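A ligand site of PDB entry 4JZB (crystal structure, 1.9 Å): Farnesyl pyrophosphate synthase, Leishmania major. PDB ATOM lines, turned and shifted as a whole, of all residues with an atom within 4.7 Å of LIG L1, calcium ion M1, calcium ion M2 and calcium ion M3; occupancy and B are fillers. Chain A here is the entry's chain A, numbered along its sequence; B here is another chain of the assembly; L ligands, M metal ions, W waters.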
ATOM      1  N   PHE A  94      24.601  -8.724 -17.720  1.00  0.00           N
ATOM      2  CA  PHE A  94      25.052  -8.288 -16.383  1.00  0.00           C
ATOM      3  C   PHE A  94      23.888  -7.810 -15.516  1.00  0.00           C
ATOM      4  O   PHE A  94      23.792  -8.179 -14.338  1.00  0.00           O
ATOM      5  CB  PHE A  94      26.103  -7.177 -16.462  1.00  0.00           C
ATOM      6  CG  PHE A  94      27.451  -7.607 -17.017  1.00  0.00           C
ATOM      7  CD1 PHE A  94      28.212  -6.719 -17.770  1.00  0.00           C
ATOM      8  CD2 PHE A  94      27.949  -8.890 -16.784  1.00  0.00           C
ATOM      9  CE1 PHE A  94      29.458  -7.088 -18.286  1.00  0.00           C
ATOM     10  CE2 PHE A  94      29.196  -9.281 -17.301  1.00  0.00           C
ATOM     11  CZ  PHE A  94      29.951  -8.372 -18.045  1.00  0.00           C
ATOM     12  N   LEU A  95      23.003  -7.007 -16.093  1.00  0.00           N
ATOM     13  CA  LEU A  95      21.907  -6.407 -15.318  1.00  0.00           C
ATOM     14  C   LEU A  95      20.865  -7.428 -14.883  1.00  0.00           C
ATOM     15  O   LEU A  95      20.354  -7.343 -13.764  1.00  0.00           O
ATOM     16  CB  LEU A  95      21.266  -5.233 -16.051  1.00  0.00           C
ATOM     17  CG  LEU A  95      22.152  -4.052 -16.473  1.00  0.00           C
ATOM     18  CD1 LEU A  95      21.287  -2.883 -16.950  1.00  0.00           C
ATOM     19  CD2 LEU A  95      23.129  -3.599 -15.385  1.00  0.00           C
ATOM     20  N   ASP A  98      22.667  -9.237 -12.096  1.00  0.00           N
ATOM     21  CA  ASP A  98      22.814  -8.308 -10.986  1.00  0.00           C
ATOM     22  C   ASP A  98      21.505  -8.060 -10.232  1.00  0.00           C
ATOM     23  O   ASP A  98      21.490  -8.038  -8.994  1.00  0.00           O
ATOM     24  CB  ASP A  98      23.372  -6.960 -11.466  1.00  0.00           C
ATOM     25  CG  ASP A  98      23.574  -5.997 -10.322  1.00  0.00           C
ATOM     26  OD1 ASP A  98      24.346  -6.331  -9.414  1.00  0.00           O
ATOM     27  OD2 ASP A  98      22.914  -4.934 -10.313  1.00  0.00           O
ATOM     28  N   ASP A  99      20.414  -7.878 -10.968  1.00  0.00           N
ATOM     29  CA  ASP A  99      19.111  -7.632 -10.338  1.00  0.00           C
ATOM     30  C   ASP A  99      18.696  -8.794  -9.441  1.00  0.00           C
ATOM     31  O   ASP A  99      18.115  -8.589  -8.384  1.00  0.00           O
ATOM     32  CB  ASP A  99      18.053  -7.258 -11.380  1.00  0.00           C
ATOM     33  CG  ASP A  99      18.228  -5.831 -11.903  1.00  0.00           C
ATOM     34  OD1 ASP A  99      18.937  -5.038 -11.249  1.00  0.00           O
ATOM     35  OD2 ASP A  99      17.669  -5.488 -12.974  1.00  0.00           O
ATOM     36  N   MET A 101      20.991 -10.930  -7.992  1.00  0.00           N
ATOM     37  CA  MET A 101      21.972 -10.903  -6.898  1.00  0.00           C
ATOM     38  C   MET A 101      21.666  -9.807  -5.868  1.00  0.00           C
ATOM     39  O   MET A 101      21.806 -10.030  -4.661  1.00  0.00           O
ATOM     40  CB  MET A 101      23.396 -10.755  -7.463  1.00  0.00           C
ATOM     41  CG  MET A 101      23.938 -12.047  -8.075  1.00  0.00           C
ATOM     42  SD  MET A 101      25.645 -11.904  -8.659  1.00  0.00           S
ATOM     43  CE  MET A 101      25.377 -11.454 -10.362  1.00  0.00           C
ATOM     44  N   ASP A 102      21.236  -8.630  -6.346  1.00  0.00           N
ATOM     45  CA  ASP A 102      20.895  -7.517  -5.444  1.00  0.00           C
ATOM     46  C   ASP A 102      19.466  -7.574  -4.904  1.00  0.00           C
ATOM     47  O   ASP A 102      19.088  -6.738  -4.073  1.00  0.00           O
ATOM     48  CB  ASP A 102      21.088  -6.177  -6.149  1.00  0.00           C
ATOM     49  CG  ASP A 102      22.557  -5.820  -6.373  1.00  0.00           C
ATOM     50  OD1 ASP A 102      23.463  -6.491  -5.836  1.00  0.00           O
ATOM     51  OD2 ASP A 102      22.793  -4.848  -7.089  1.00  0.00           O
ATOM     52  N   SER A 104      16.728  -6.803  -6.499  1.00  0.00           N
ATOM     53  CA  SER A 104      16.175  -5.499  -6.850  1.00  0.00           C
ATOM     54  C   SER A 104      14.742  -5.557  -7.370  1.00  0.00           C
ATOM     55  O   SER A 104      14.247  -6.617  -7.756  1.00  0.00           O
ATOM     56  CB  SER A 104      17.086  -4.803  -7.864  1.00  0.00           C
ATOM     57  OG  SER A 104      18.342  -4.515  -7.279  1.00  0.00           O
ATOM     58  N   ARG A 107      14.064  -1.872 -12.902  1.00  0.00           N
ATOM     59  CA  ARG A 107      15.165  -1.594 -13.829  1.00  0.00           C
ATOM     60  C   ARG A 107      14.611  -0.858 -15.041  1.00  0.00           C
ATOM     61  O   ARG A 107      13.654  -1.325 -15.656  1.00  0.00           O
ATOM     62  CB  ARG A 107      15.827  -2.914 -14.285  1.00  0.00           C
ATOM     63  CG  ARG A 107      16.836  -2.752 -15.443  1.00  0.00           C
ATOM     64  CD  ARG A 107      18.130  -2.062 -14.996  1.00  0.00           C
ATOM     65  NE  ARG A 107      18.921  -2.858 -14.060  1.00  0.00           N
ATOM     66  CZ  ARG A 107      20.009  -2.415 -13.433  1.00  0.00           C
ATOM     67  NH1 ARG A 107      20.430  -1.182 -13.644  1.00  0.00           N
ATOM     68  NH2 ARG A 107      20.669  -3.201 -12.599  1.00  0.00           N
ATOM     69  N   THR A 163      35.028  -7.878 -15.710  1.00  0.00           N
ATOM     70  CA  THR A 163      33.791  -7.455 -15.043  1.00  0.00           C
ATOM     71  C   THR A 163      33.328  -8.439 -13.959  1.00  0.00           C
ATOM     72  O   THR A 163      32.861  -8.012 -12.888  1.00  0.00           O
ATOM     73  CB  THR A 163      32.674  -7.198 -16.076  1.00  0.00           C
ATOM     74  OG1 THR A 163      33.196  -6.420 -17.163  1.00  0.00           O
ATOM     75  CG2 THR A 163      31.525  -6.447 -15.436  1.00  0.00           C
ATOM     76  N   GLN A 167      32.833  -7.753 -10.105  1.00  0.00           N
ATOM     77  CA  GLN A 167      31.640  -8.199  -9.362  1.00  0.00           C
ATOM     78  C   GLN A 167      31.993  -9.039  -8.110  1.00  0.00           C
ATOM     79  O   GLN A 167      31.340  -8.900  -7.075  1.00  0.00           O
ATOM     80  CB  GLN A 167      30.640  -8.912 -10.278  1.00  0.00           C
ATOM     81  CG  GLN A 167      29.338  -9.342  -9.583  1.00  0.00           C
ATOM     82  CD  GLN A 167      28.470  -8.175  -9.107  1.00  0.00           C
ATOM     83  OE1 GLN A 167      28.839  -7.008  -9.235  1.00  0.00           O
ATOM     84  NE2 GLN A 167      27.295  -8.498  -8.559  1.00  0.00           N
ATOM     85  N   ASP A 170      32.880  -6.581  -5.542  1.00  0.00           N
ATOM     86  CA  ASP A 170      31.633  -5.949  -5.088  1.00  0.00           C
ATOM     87  C   ASP A 170      30.862  -6.798  -4.060  1.00  0.00           C
ATOM     88  O   ASP A 170      30.503  -6.305  -2.977  1.00  0.00           O
ATOM     89  CB  ASP A 170      30.758  -5.628  -6.308  1.00  0.00           C
ATOM     90  CG  ASP A 170      29.456  -4.937  -5.919  1.00  0.00           C
ATOM     91  OD1 ASP A 170      29.332  -3.729  -6.206  1.00  0.00           O
ATOM     92  OD2 ASP A 170      28.565  -5.595  -5.333  1.00  0.00           O
ATOM     93  N   LYS A 207      34.521  -3.619 -12.203  1.00  0.00           N
ATOM     94  CA  LYS A 207      33.109  -3.957 -12.455  1.00  0.00           C
ATOM     95  C   LYS A 207      32.466  -3.042 -13.499  1.00  0.00           C
ATOM     96  O   LYS A 207      31.460  -3.416 -14.096  1.00  0.00           O
ATOM     97  CB  LYS A 207      32.269  -4.011 -11.158  1.00  0.00           C
ATOM     98  CG  LYS A 207      31.683  -2.667 -10.667  1.00  0.00           C
ATOM     99  CD  LYS A 207      30.595  -2.860  -9.585  1.00  0.00           C
ATOM    100  CE  LYS A 207      30.032  -1.509  -9.138  1.00  0.00           C
ATOM    101  NZ  LYS A 207      29.064  -1.622  -7.970  1.00  0.00           N
ATOM    102  N   THR A 208      33.037  -1.853 -13.722  1.00  0.00           N
ATOM    103  CA  THR A 208      32.384  -0.864 -14.590  1.00  0.00           C
ATOM    104  C   THR A 208      33.239  -0.278 -15.706  1.00  0.00           C
ATOM    105  O   THR A 208      32.819  -0.245 -16.864  1.00  0.00           O
ATOM    106  CB  THR A 208      31.753   0.277 -13.750  1.00  0.00           C
ATOM    107  OG1 THR A 208      30.708  -0.286 -12.948  1.00  0.00           O
ATOM    108  CG2 THR A 208      31.187   1.419 -14.631  1.00  0.00           C
ATOM    109  N   TYR A 211      34.058  -2.510 -19.199  1.00  0.00           N
ATOM    110  CA  TYR A 211      32.973  -2.783 -20.133  1.00  0.00           C
ATOM    111  C   TYR A 211      32.188  -1.536 -20.569  1.00  0.00           C
ATOM    112  O   TYR A 211      31.566  -1.548 -21.633  1.00  0.00           O
ATOM    113  CB  TYR A 211      32.063  -3.906 -19.625  1.00  0.00           C
ATOM    114  CG  TYR A 211      30.852  -3.515 -18.812  1.00  0.00           C
ATOM    115  CD1 TYR A 211      29.588  -3.403 -19.420  1.00  0.00           C
ATOM    116  CD2 TYR A 211      30.935  -3.300 -17.435  1.00  0.00           C
ATOM    117  CE1 TYR A 211      28.456  -3.074 -18.676  1.00  0.00           C
ATOM    118  CE2 TYR A 211      29.797  -2.972 -16.682  1.00  0.00           C
ATOM    119  CZ  TYR A 211      28.569  -2.854 -17.313  1.00  0.00           C
ATOM    120  OH  TYR A 211      27.443  -2.525 -16.577  1.00  0.00           O
ATOM    121  N   GLN A 247      30.921   5.370 -12.391  1.00  0.00           N
ATOM    122  CA  GLN A 247      30.406   4.560 -11.287  1.00  0.00           C
ATOM    123  C   GLN A 247      30.231   5.340  -9.979  1.00  0.00           C
ATOM    124  O   GLN A 247      29.308   5.070  -9.205  1.00  0.00           O
ATOM    125  CB  GLN A 247      31.256   3.324 -11.042  1.00  0.00           C
ATOM    126  CG  GLN A 247      30.627   2.350 -10.049  1.00  0.00           C
ATOM    127  CD  GLN A 247      29.269   1.818 -10.512  1.00  0.00           C
ATOM    128  OE1 GLN A 247      29.106   1.460 -11.668  1.00  0.00           O
ATOM    129  NE2 GLN A 247      28.304   1.778  -9.606  1.00  0.00           N
ATOM    130  N   ASP A 250      26.983   6.891 -10.390  1.00  0.00           N
ATOM    131  CA  ASP A 250      25.976   5.874 -10.093  1.00  0.00           C
ATOM    132  C   ASP A 250      25.778   5.705  -8.576  1.00  0.00           C
ATOM    133  O   ASP A 250      24.632   5.651  -8.106  1.00  0.00           O
ATOM    134  CB  ASP A 250      26.335   4.535 -10.750  1.00  0.00           C
ATOM    135  CG  ASP A 250      25.200   3.541 -10.680  1.00  0.00           C
ATOM    136  OD1 ASP A 250      24.175   3.755 -11.362  1.00  0.00           O
ATOM    137  OD2 ASP A 250      25.337   2.534  -9.940  1.00  0.00           O
ATOM    138  N   LYS A 264      15.423   2.993 -11.383  1.00  0.00           N
ATOM    139  CA  LYS A 264      15.795   1.829 -10.568  1.00  0.00           C
ATOM    140  C   LYS A 264      15.804   2.222  -9.099  1.00  0.00           C
ATOM    141  O   LYS A 264      15.991   3.399  -8.784  1.00  0.00           O
ATOM    142  CB  LYS A 264      17.171   1.270 -10.993  1.00  0.00           C
ATOM    143  CG  LYS A 264      18.364   2.225 -10.777  1.00  0.00           C
ATOM    144  CD  LYS A 264      19.598   1.758 -11.538  1.00  0.00           C
ATOM    145  CE  LYS A 264      20.797   2.654 -11.231  1.00  0.00           C
ATOM    146  NZ  LYS A 264      21.939   2.432 -12.178  1.00  0.00           N
ATOM    147  N   ASP A 268      21.951   0.416  -1.816  1.00  0.00           N
ATOM    148  CA  ASP A 268      23.340   0.442  -1.344  1.00  0.00           C
ATOM    149  C   ASP A 268      23.409   0.599   0.172  1.00  0.00           C
ATOM    150  O   ASP A 268      24.232  -0.029   0.838  1.00  0.00           O
ATOM    151  CB  ASP A 268      24.127   1.579  -1.999  1.00  0.00           C
ATOM    152  CG  ASP A 268      24.517   1.276  -3.441  1.00  0.00           C
ATOM    153  OD1 ASP A 268      24.224   0.169  -3.950  1.00  0.00           O
ATOM    154  OD2 ASP A 268      25.128   2.171  -4.083  1.00  0.00           O
ATOM    155  N   ASN B 126      27.523 -15.296  -9.685  1.00  0.00           N
ATOM    156  CA  ASN B 126      28.712 -14.675 -10.282  1.00  0.00           C
ATOM    157  C   ASN B 126      29.935 -15.600 -10.325  1.00  0.00           C
ATOM    158  O   ASN B 126      30.710 -15.534 -11.278  1.00  0.00           O
ATOM    159  CB  ASN B 126      29.069 -13.363  -9.596  1.00  0.00           C
ATOM    160  CG  ASN B 126      30.134 -12.584 -10.358  1.00  0.00           C
ATOM    161  OD1 ASN B 126      29.900 -12.128 -11.473  1.00  0.00           O
ATOM    162  ND2 ASN B 126      31.304 -12.448  -9.760  1.00  0.00           N
ATOM    163  N   LEU B 129      29.761 -17.366 -13.440  1.00  0.00           N
ATOM    164  CA  LEU B 129      30.171 -16.535 -14.575  1.00  0.00           C
ATOM    165  C   LEU B 129      31.686 -16.462 -14.702  1.00  0.00           C
ATOM    166  O   LEU B 129      32.214 -16.453 -15.815  1.00  0.00           O
ATOM    167  CB  LEU B 129      29.601 -15.124 -14.462  1.00  0.00           C
ATOM    168  CG  LEU B 129      28.079 -14.942 -14.339  1.00  0.00           C
ATOM    169  CD1 LEU B 129      27.735 -13.459 -14.388  1.00  0.00           C
ATOM    170  CD2 LEU B 129      27.371 -15.695 -15.436  1.00  0.00           C
HETATM  171  C1  LIG L   1      24.825  -2.443 -11.740  1.00  0.00           C
HETATM  172  C2  LIG L   1      24.723  -1.302 -10.712  1.00  0.00           C
HETATM  173  P1  LIG L   1      25.377  -1.781  -9.076  1.00  0.00           P
HETATM  174  O1  LIG L   1      24.538  -2.891  -8.499  1.00  0.00           O
HETATM  175  O2  LIG L   1      25.316  -0.512  -8.251  1.00  0.00           O
HETATM  176  N1  LIG L   1      26.148  -2.969 -12.103  1.00  0.00           N
HETATM  177  O3  LIG L   1      26.800  -2.208  -9.291  1.00  0.00           O
HETATM  178  C3  LIG L   1      27.212  -2.158 -12.341  1.00  0.00           C
HETATM  179  O4  LIG L   1      25.500  -0.159 -11.158  1.00  0.00           O
HETATM  180  C4  LIG L   1      28.445  -2.684 -12.698  1.00  0.00           C
HETATM  181  P2  LIG L   1      22.959  -0.811 -10.725  1.00  0.00           P
HETATM  182  C5  LIG L   1      28.598  -4.070 -12.820  1.00  0.00           C
HETATM  183  O5  LIG L   1      22.823   0.329  -9.749  1.00  0.00           O
HETATM  184  C6  LIG L   1      27.497  -4.905 -12.573  1.00  0.00           C
HETATM  185  O6  LIG L   1      22.189  -2.046 -10.317  1.00  0.00           O
HETATM  186  C7  LIG L   1      26.280  -4.302 -12.225  1.00  0.00           C
HETATM  187  O7  LIG L   1      22.661  -0.403 -12.161  1.00  0.00           O
HETATM  188  C8  LIG L   1      27.610  -6.390 -12.694  1.00  0.00           C
HETATM  189  C9  LIG L   1      28.576  -6.964 -13.519  1.00  0.00           C
HETATM  190  C10 LIG L   1      28.686  -8.351 -13.624  1.00  0.00           C
HETATM  191  C11 LIG L   1      27.819  -9.191 -12.913  1.00  0.00           C
HETATM  192  C12 LIG L   1      26.839  -8.613 -12.086  1.00  0.00           C
HETATM  193  C13 LIG L   1      26.760  -7.231 -11.970  1.00  0.00           C
HETATM  194  C1  LG2 L   2      24.115   0.780 -15.182  1.00  0.00           C
HETATM  195  O1  LG2 L   2      24.586   1.237 -16.455  1.00  0.00           O
HETATM  196  C2  LG2 L   2      25.204  -0.027 -14.482  1.00  0.00           C
HETATM  197  C3  LG2 L   2      26.465   0.779 -14.246  1.00  0.00           C
HETATM  198  C4  LG2 L   2      26.460   1.863 -13.476  1.00  0.00           C
HETATM  199  C5  LG2 L   2      27.741   0.335 -14.870  1.00  0.00           C
HETATM  200  P1  LG2 L   2      23.810   2.389 -17.257  1.00  0.00           P
HETATM  201  O2  LG2 L   2      24.631   2.691 -18.493  1.00  0.00           O
HETATM  202  O3  LG2 L   2      23.496   3.531 -16.307  1.00  0.00           O
HETATM  203  O4  LG2 L   2      22.408   1.663 -17.612  1.00  0.00           O
HETATM  204  P2  LG2 L   2      21.550   1.715 -18.987  1.00  0.00           P
HETATM  205  O5  LG2 L   2      21.725   3.090 -19.615  1.00  0.00           O
HETATM  206  O6  LG2 L   2      22.164   0.590 -19.789  1.00  0.00           O
HETATM  207  O7  LG2 L   2      20.160   1.443 -18.466  1.00  0.00           O
HETATM  208 CA    CA M   1      22.284  -3.459  -8.752  1.00  0.00          CA
HETATM  209 CA    CA M   2      25.161  -4.998  -7.665  1.00  0.00          CA
HETATM  210 CA    CA M   3      24.176   1.421  -8.214  1.00  0.00          CA
HETATM  211  O   HOH W   1      22.835   3.526  -8.417  1.00  0.00           O
HETATM  212  O   HOH W   2      22.893   0.972  -6.269  1.00  0.00           O
HETATM  213  O   HOH W   3      26.403  -6.871  -6.509  1.00  0.00           O
HETATM  214  O   HOH W   4      27.132  -4.872  -8.883  1.00  0.00           O
HETATM  215  O   HOH W   5      20.439   0.651  -8.425  1.00  0.00           O
HETATM  216  O   HOH W   6      25.676   2.279  -6.577  1.00  0.00           O
HETATM  217  O   HOH W   7      26.268  -3.693  -6.006  1.00  0.00           O
HETATM  218  O   HOH W   8      26.059  -1.030  -5.629  1.00  0.00           O
HETATM  219  O   HOH W   9      21.490  -1.897  -7.214  1.00  0.00           O
HETATM  220  O   HOH W  10      20.209  -4.272  -9.031  1.00  0.00           O
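Water W10 bridges the side-chain hydroxyl of Ser 104 (2.6 Å) and the side-chain carboxylate of Asp 99 (2.7 Å). Water W4 lies within hydrogen-bond range of O3 of LIG L1 and OE1 of Gln 167. Water W3 lies within hydrogen-bond range of the side-chain amide nitrogen (NE2) of Gln 167 (2.8 Å), the side-chain carboxylate (OD2) of Asp 170 (2.8 Å) and the side-chain carboxylate (OD1) of Asp 102 (3.0 Å).
NZ of Lys 207 is in salt-bridge range of O3 of LIG L1 (2.7 Å). The guanidinium group of Arg 107 is in salt-bridge range of an oxygen (O7) of LIG L1. An oxygen (O7) of LIG L1 is in salt-bridge range of the side-chain amino group of Lys 264.
The side-chain carboxylate of Asp 98 lies close to the guanidinium group of Arg 107 (3.6 Å). The side-chain amino group (NZ) of Lys 264 lies within salt-bridge range of the side-chain carboxylate (OD1) of Asp 250. NE2 of Gln 247 lies close to OD2 of Asp 250 (3.1 Å). OD1 of Asp 170 is in salt-bridge range of NZ of Lys 207. The side-chain carboxylate (OD1) of Asp 99 is in salt-bridge range of the guanidinium group (NH2) of Arg 107, 2.9 Å away. OG1 of Thr 208 is in hydrogen-bond range of OE1 of Gln 247, 2.7 Å away. The side-chain amide nitrogen of Gln 167 is in hydrogen-bond range of the side-chain sulfur of Met 101, 3.8 Å away.
Within 4 Å of calcium ion M1: Asp 98 and Asp 102.
Calcium ion M1 is bound by an oxygen (O6) of LIG L1 (2.1 Å), the side-chain carboxylate (OD2) of Asp 102 (2.2 Å), the side-chain carboxylate (OD2) of Asp 98 (2.2 Å), water W10 (2.2 Å), water W9 (2.3 Å) and an oxygen (O1) of LIG L1 (2.3 Å).
Phe 94 touches LIG L1 (CD2 to C10, 3.3 Å). Met 101 touches LIG L1 (CE to C12, 3.6 Å). CG2 of Thr 163 touches C9 of LIG L1, 3.6 Å away. Gln 167 touches LIG L1 (CD to C12, 3.4 Å). OG1 of Thr 208 touches C4 of LIG L1, at 3.3 Å. Gln 247 touches LIG L1. OD1 of Asn 126 of chain B touches C11 of LIG L1, 3.9 Å away. Of the 20 residues printed, 13 come within 4 Å of LIG L1.
Calcium ion M3 is bound by an oxygen (O2) of LIG L1 (2.2 Å), an oxygen (O5) of LIG L1 (2.3 Å), the side-chain carboxylate of Asp 250 (2.4 Å), water W2 (2.4 Å), water W6 (2.4 Å) and water W1 (2.5 Å).
Water W4 is bound to calcium ion M2 (2.3 Å). OD1 of Asp 98 is bound to calcium ion M2 (2.3 Å). O1 of LIG L1 binds calcium ion M2. Calcium ion M2 is bound by water W7. OD2 of Asp 102 is bound to calcium ion M2 (2.4 Å). Water W3 is bound to calcium ion M2, at 2.5 Å. Slightly farther from calcium ion M2 lies OD1 of Asp 102 (2.9 Å).
Of the 20 residues printed, 1 comes within 4 Å of calcium ion M3. The nearest printed residue that does not touch calcium ion M3 is Asp 268 (4.3 Å).
Two residues have an atom within 4 Å of calcium ion M2: Asp 98 and Asp 102. Along chain A the residues within 4 Å of calcium ion M2 span positions 98 to 102. The nearest printed residue that does not touch calcium ion M2 is Asp 170 (4.2 Å).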
